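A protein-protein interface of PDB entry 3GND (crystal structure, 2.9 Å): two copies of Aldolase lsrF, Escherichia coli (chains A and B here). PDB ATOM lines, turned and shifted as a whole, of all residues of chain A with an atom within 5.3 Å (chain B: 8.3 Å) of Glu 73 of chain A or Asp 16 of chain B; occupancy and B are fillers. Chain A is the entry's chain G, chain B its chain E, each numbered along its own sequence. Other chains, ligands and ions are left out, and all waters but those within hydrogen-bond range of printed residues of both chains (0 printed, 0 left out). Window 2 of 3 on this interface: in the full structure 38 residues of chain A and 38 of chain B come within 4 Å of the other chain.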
ATOM      1  N   PRO A  68     -27.118  -2.668 -20.263  1.00  0.00           N
ATOM      2  CA  PRO A  68     -26.763  -4.037 -19.948  1.00  0.00           C
ATOM      3  C   PRO A  68     -27.977  -4.908 -20.093  1.00  0.00           C
ATOM      4  O   PRO A  68     -28.688  -5.113 -19.121  1.00  0.00           O
ATOM      5  CB  PRO A  68     -26.363  -3.985 -18.468  1.00  0.00           C
ATOM      6  CG  PRO A  68     -26.379  -2.564 -18.067  1.00  0.00           C
ATOM      7  CD  PRO A  68     -27.231  -1.844 -19.051  1.00  0.00           C
ATOM      8  N   THR A  69     -28.226  -5.394 -21.301  1.00  0.00           N
ATOM      9  CA  THR A  69     -29.268  -6.377 -21.593  1.00  0.00           C
ATOM     10  C   THR A  69     -28.914  -7.755 -20.995  1.00  0.00           C
ATOM     11  O   THR A  69     -27.741  -8.053 -20.753  1.00  0.00           O
ATOM     12  CB  THR A  69     -29.430  -6.491 -23.120  1.00  0.00           C
ATOM     13  OG1 THR A  69     -30.524  -7.333 -23.428  1.00  0.00           O
ATOM     14  CG2 THR A  69     -28.191  -7.094 -23.768  1.00  0.00           C
ATOM     15  N   THR A  70     -29.921  -8.588 -20.735  1.00  0.00           N
ATOM     16  CA  THR A  70     -29.696  -9.925 -20.146  1.00  0.00           C
ATOM     17  C   THR A  70     -28.782 -10.807 -20.978  1.00  0.00           C
ATOM     18  O   THR A  70     -29.038 -10.984 -22.154  1.00  0.00           O
ATOM     19  CB  THR A  70     -30.985 -10.697 -20.008  1.00  0.00           C
ATOM     20  OG1 THR A  70     -31.845  -9.962 -19.162  1.00  0.00           O
ATOM     21  CG2 THR A  70     -30.726 -12.008 -19.361  1.00  0.00           C
ATOM     22  N   GLY A  71     -27.746 -11.383 -20.367  1.00  0.00           N
ATOM     23  CA  GLY A  71     -26.784 -12.194 -21.094  1.00  0.00           C
ATOM     24  C   GLY A  71     -25.540 -11.422 -21.527  1.00  0.00           C
ATOM     25  O   GLY A  71     -24.492 -12.036 -21.823  1.00  0.00           O
ATOM     26  N   LEU A  72     -25.655 -10.085 -21.564  1.00  0.00           N
ATOM     27  CA  LEU A  72     -24.570  -9.206 -21.980  1.00  0.00           C
ATOM     28  C   LEU A  72     -24.125  -8.263 -20.858  1.00  0.00           C
ATOM     29  O   LEU A  72     -23.492  -7.213 -21.098  1.00  0.00           O
ATOM     30  CB  LEU A  72     -24.968  -8.411 -23.204  1.00  0.00           C
ATOM     31  CG  LEU A  72     -25.414  -9.246 -24.397  1.00  0.00           C
ATOM     32  CD1 LEU A  72     -25.921  -8.350 -25.526  1.00  0.00           C
ATOM     33  CD2 LEU A  72     -24.279 -10.139 -24.886  1.00  0.00           C
ATOM     34  N   GLU A  73     -24.436  -8.631 -19.620  1.00  0.00           N
ATOM     35  CA  GLU A  73     -23.937  -7.856 -18.495  1.00  0.00           C
ATOM     36  C   GLU A  73     -22.419  -7.878 -18.518  1.00  0.00           C
ATOM     37  O   GLU A  73     -21.797  -6.846 -18.353  1.00  0.00           O
ATOM     38  CB  GLU A  73     -24.450  -8.412 -17.166  1.00  0.00           C
ATOM     39  CG  GLU A  73     -25.955  -8.517 -17.054  1.00  0.00           C
ATOM     40  CD  GLU A  73     -26.500  -9.825 -17.585  1.00  0.00           C
ATOM     41  OE1 GLU A  73     -25.799 -10.494 -18.365  1.00  0.00           O
ATOM     42  OE2 GLU A  73     -27.638 -10.187 -17.228  1.00  0.00           O
ATOM     43  N   ARG A  74     -21.837  -9.061 -18.722  1.00  0.00           N
ATOM     44  CA  ARG A  74     -20.395  -9.200 -18.715  1.00  0.00           C
ATOM     45  C   ARG A  74     -19.838  -9.836 -20.010  1.00  0.00           C
ATOM     46  O   ARG A  74     -19.507 -11.026 -20.025  1.00  0.00           O
ATOM     47  CB  ARG A  74     -19.943  -9.967 -17.477  1.00  0.00           C
ATOM     48  CG  ARG A  74     -20.326  -9.299 -16.176  1.00  0.00           C
ATOM     49  CD  ARG A  74     -19.501  -8.032 -15.883  1.00  0.00           C
ATOM     50  NE  ARG A  74     -18.057  -8.262 -15.878  1.00  0.00           N
ATOM     51  CZ  ARG A  74     -17.390  -8.697 -14.826  1.00  0.00           C
ATOM     52  NH1 ARG A  74     -18.048  -8.946 -13.713  1.00  0.00           N
ATOM     53  NH2 ARG A  74     -16.087  -8.884 -14.880  1.00  0.00           N
ATOM     54  N   ILE A  75     -19.717  -9.029 -21.071  1.00  0.00           N
ATOM     55  CA  ILE A  75     -19.170  -9.485 -22.331  1.00  0.00           C
ATOM     56  C   ILE A  75     -17.831 -10.142 -22.057  1.00  0.00           C
ATOM     57  O   ILE A  75     -17.508 -11.204 -22.624  1.00  0.00           O
ATOM     58  CB  ILE A  75     -18.928  -8.308 -23.303  1.00  0.00           C
ATOM     59  CG1 ILE A  75     -20.202  -7.454 -23.482  1.00  0.00           C
ATOM     60  CG2 ILE A  75     -18.362  -8.796 -24.648  1.00  0.00           C
ATOM     61  CD1 ILE A  75     -21.249  -8.066 -24.352  1.00  0.00           C
ATOM     62  N   ASN A  78     -18.802 -13.784 -20.228  1.00  0.00           N
ATOM     63  CA  ASN A  78     -19.715 -14.703 -20.890  1.00  0.00           C
ATOM     64  C   ASN A  78     -19.512 -14.788 -22.400  1.00  0.00           C
ATOM     65  O   ASN A  78     -19.626 -15.866 -22.973  1.00  0.00           O
ATOM     66  CB  ASN A  78     -21.175 -14.339 -20.607  1.00  0.00           C
ATOM     67  CG  ASN A  78     -21.534 -14.486 -19.150  1.00  0.00           C
ATOM     68  OD1 ASN A  78     -20.691 -14.847 -18.322  1.00  0.00           O
ATOM     69  ND2 ASN A  78     -22.789 -14.200 -18.817  1.00  0.00           N
ATOM     70  N   GLY B  14     -33.706 -10.781 -12.944  1.00  0.00           N
ATOM     71  CA  GLY B  14     -33.093 -12.001 -13.557  1.00  0.00           C
ATOM     72  C   GLY B  14     -31.796 -11.729 -14.312  1.00  0.00           C
ATOM     73  O   GLY B  14     -31.572 -12.275 -15.391  1.00  0.00           O
ATOM     74  N   LYS B  15     -30.935 -10.890 -13.744  1.00  0.00           N
ATOM     75  CA  LYS B  15     -29.671 -10.549 -14.372  1.00  0.00           C
ATOM     76  C   LYS B  15     -28.498 -10.944 -13.482  1.00  0.00           C
ATOM     77  O   LYS B  15     -28.588 -10.865 -12.258  1.00  0.00           O
ATOM     78  CB  LYS B  15     -29.618  -9.050 -14.677  1.00  0.00           C
ATOM     79  CG  LYS B  15     -30.598  -8.631 -15.745  1.00  0.00           C
ATOM     80  CD  LYS B  15     -30.391  -7.210 -16.231  1.00  0.00           C
ATOM     81  CE  LYS B  15     -31.351  -6.961 -17.363  1.00  0.00           C
ATOM     82  NZ  LYS B  15     -31.441  -5.554 -17.694  1.00  0.00           N
ATOM     83  N   ASP B  16     -27.395 -11.362 -14.101  1.00  0.00           N
ATOM     84  CA  ASP B  16     -26.195 -11.712 -13.353  1.00  0.00           C
ATOM     85  C   ASP B  16     -24.990 -10.877 -13.788  1.00  0.00           C
ATOM     86  O   ASP B  16     -24.387 -11.149 -14.826  1.00  0.00           O
ATOM     87  CB  ASP B  16     -25.899 -13.200 -13.528  1.00  0.00           C
ATOM     88  CG  ASP B  16     -24.813 -13.693 -12.606  1.00  0.00           C
ATOM     89  OD1 ASP B  16     -24.444 -12.989 -11.651  1.00  0.00           O
ATOM     90  OD2 ASP B  16     -24.331 -14.807 -12.838  1.00  0.00           O
ATOM     91  N   PHE B  17     -24.642  -9.867 -12.990  1.00  0.00           N
ATOM     92  CA  PHE B  17     -23.518  -8.977 -13.300  1.00  0.00           C
ATOM     93  C   PHE B  17     -22.206  -9.512 -12.795  1.00  0.00           C
ATOM     94  O   PHE B  17     -21.182  -8.843 -12.894  1.00  0.00           O
ATOM     95  CB  PHE B  17     -23.735  -7.585 -12.710  1.00  0.00           C
ATOM     96  CG  PHE B  17     -24.803  -6.798 -13.411  1.00  0.00           C
ATOM     97  CD1 PHE B  17     -24.484  -5.945 -14.434  1.00  0.00           C
ATOM     98  CD2 PHE B  17     -26.122  -6.924 -13.057  1.00  0.00           C
ATOM     99  CE1 PHE B  17     -25.455  -5.234 -15.074  1.00  0.00           C
ATOM    100  CE2 PHE B  17     -27.082  -6.218 -13.704  1.00  0.00           C
ATOM    101  CZ  PHE B  17     -26.751  -5.380 -14.711  1.00  0.00           C
ATOM    102  N   ARG B  18     -22.252 -10.727 -12.258  1.00  0.00           N
ATOM    103  CA  ARG B  18     -21.099 -11.359 -11.632  1.00  0.00           C
ATOM    104  C   ARG B  18     -20.176 -10.349 -10.913  1.00  0.00           C
ATOM    105  O   ARG B  18     -19.013 -10.203 -11.256  1.00  0.00           O
ATOM    106  CB  ARG B  18     -20.347 -12.203 -12.656  1.00  0.00           C
ATOM    107  CG  ARG B  18     -19.551 -13.337 -12.000  1.00  0.00           C
ATOM    108  CD  ARG B  18     -19.432 -14.540 -12.919  1.00  0.00           C
ATOM    109  NE  ARG B  18     -20.654 -14.675 -13.706  1.00  0.00           N
ATOM    110  CZ  ARG B  18     -20.795 -15.513 -14.723  1.00  0.00           C
ATOM    111  NH1 ARG B  18     -19.787 -16.287 -15.072  1.00  0.00           N
ATOM    112  NH2 ARG B  18     -21.937 -15.576 -15.391  1.00  0.00           N
ATOM    113  N   THR B  19     -20.704  -9.672  -9.895  1.00  0.00           N
ATOM    114  CA  THR B  19     -19.984  -8.578  -9.285  1.00  0.00           C
ATOM    115  C   THR B  19     -18.902  -9.071  -8.361  1.00  0.00           C
ATOM    116  O   THR B  19     -18.166  -8.277  -7.794  1.00  0.00           O
ATOM    117  CB  THR B  19     -20.929  -7.619  -8.527  1.00  0.00           C
ATOM    118  OG1 THR B  19     -21.458  -8.273  -7.380  1.00  0.00           O
ATOM    119  CG2 THR B  19     -22.077  -7.184  -9.403  1.00  0.00           C
ATOM    120  N   ASP B  20     -18.800 -10.383  -8.205  1.00  0.00           N
ATOM    121  CA  ASP B  20     -17.791 -10.946  -7.315  1.00  0.00           C
ATOM    122  C   ASP B  20     -16.503 -11.163  -8.074  1.00  0.00           C
ATOM    123  O   ASP B  20     -15.495 -11.547  -7.505  1.00  0.00           O
ATOM    124  CB  ASP B  20     -18.281 -12.255  -6.695  1.00  0.00           C
ATOM    125  CG  ASP B  20     -18.899 -13.191  -7.718  1.00  0.00           C
ATOM    126  OD1 ASP B  20     -18.420 -13.263  -8.851  1.00  0.00           O
ATOM    127  OD2 ASP B  20     -19.879 -13.871  -7.406  1.00  0.00           O
ATOM    128  N   GLN B  23     -13.431  -7.291 -13.691  1.00  0.00           N
ATOM    129  CA  GLN B  23     -12.961  -7.360 -15.068  1.00  0.00           C
ATOM    130  C   GLN B  23     -11.460  -7.127 -15.135  1.00  0.00           C
ATOM    131  O   GLN B  23     -10.947  -6.272 -14.461  1.00  0.00           O
ATOM    132  CB  GLN B  23     -13.725  -6.331 -15.891  1.00  0.00           C
ATOM    133  CG  GLN B  23     -13.232  -6.070 -17.286  1.00  0.00           C
ATOM    134  CD  GLN B  23     -13.923  -4.864 -17.915  1.00  0.00           C
ATOM    135  OE1 GLN B  23     -15.068  -4.539 -17.592  1.00  0.00           O
ATOM    136  NE2 GLN B  23     -13.220  -4.197 -18.825  1.00  0.00           N
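No position is printed for both chains. Of the 10 pairs that touch across the chains among the printed residues, none has its exchanged pair printed and touching as well.
The side-chain carboxylate (OD2) of Asp 16 of chain B lies within salt-bridge range of the guanidinium group (NH2) of Arg 18 of chain B, 3.6 Å away. N of Gly 71 of chain A lies within hydrogen-bond range of OE1 of Glu 73 of chain A, 2.9 Å away.
Of the printed residues of chain B, Pro 68 of chain A touches Lys 15 (3.1 Å) and Phe 17 (3.7 Å). Of the printed residues of chain B, Thr 70 of chain A touches Lys 15. No residue of chain B comes within 4 Å of Gly 71 of chain A. Of the printed residues of chain B, Glu 73 of chain A touches Lys 15, Asp 16 and Phe 17. Ile 75 of chain A touches none of the printed residues of chain B. Printed residues of chain B within 4 Å of Asn 78 of chain A: Arg 18. Of the printed residues of chain A, Phe 17 of chain B touches Pro 68, Glu 73 and Arg 74. Of the printed residues of chain A, Gln 23 of chain B touches Arg 74 (3.3 Å). The nearest residue of chain B that does not touch Glu 73 of chain A is Gly 14 of chain B (4.8 Å). The nearest residue of chain A that does not touch Asp 16 of chain B is Arg 74 of chain A (4.7 Å). The nearest printed residue of chain A that does not touch Lys 15 of chain B is Thr 69 of chain A (4.4 Å).
O of Pro 68 of chain A is in hydrogen-bond range of NZ of Lys 15 of chain B (3.1 Å). The side-chain carboxylate of Glu 73 of chain A is in hydrogen-bond range of the backbone NH of Asp 16 of chain B (3.3 Å). O of Phe 17 of chain B lies within hydrogen-bond range of NH1 of Arg 74 of chain A, 3.2 Å away. The backbone carbonyl oxygen (O) of Arg 18 of chain B lies within hydrogen-bond range of the guanidinium group (NH1) of Arg 74 of chain A (2.9 Å). The guanidinium group (NH2) of Arg 18 of chain B sits at hydrogen-bond distance from the side-chain amide oxygen (OD1) of Asn 78 of chain A (3.3 Å). The guanidinium group (NH2) of Arg 74 of chain A sits close to the backbone NH (N) of Gln 23 of chain B (3.3 Å).
Of the 9 printed residues of chain A, 5 touch a printed residue of chain B. Hydrophobic or aromatic side chains of chain A that line the printed part of chain B: Pro 68. Printed residues of chain B that touch a printed residue of chain A: Lys 15, Asp 16, Phe 17, Arg 18 and Gln 23. Hydrophobic or aromatic side chains of chain B within 4 Å of the printed part of chain A: Phe 17. Among the printed residues, 10 pairs touch across the chains. Among the printed residues, no Asp or Glu carboxylate lies within 4 Å of a Lys or Arg side-chain nitrogen of the other chain.
Among the printed residues, merely in contact across the chains: Pro 68 of chain A with Phe 17 of chain B, Thr 70 of chain A with Lys 15 of chain B, Glu 73 of chain A with Lys 15 of chain B and Glu 73 of chain A with Phe 17 of chain B.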
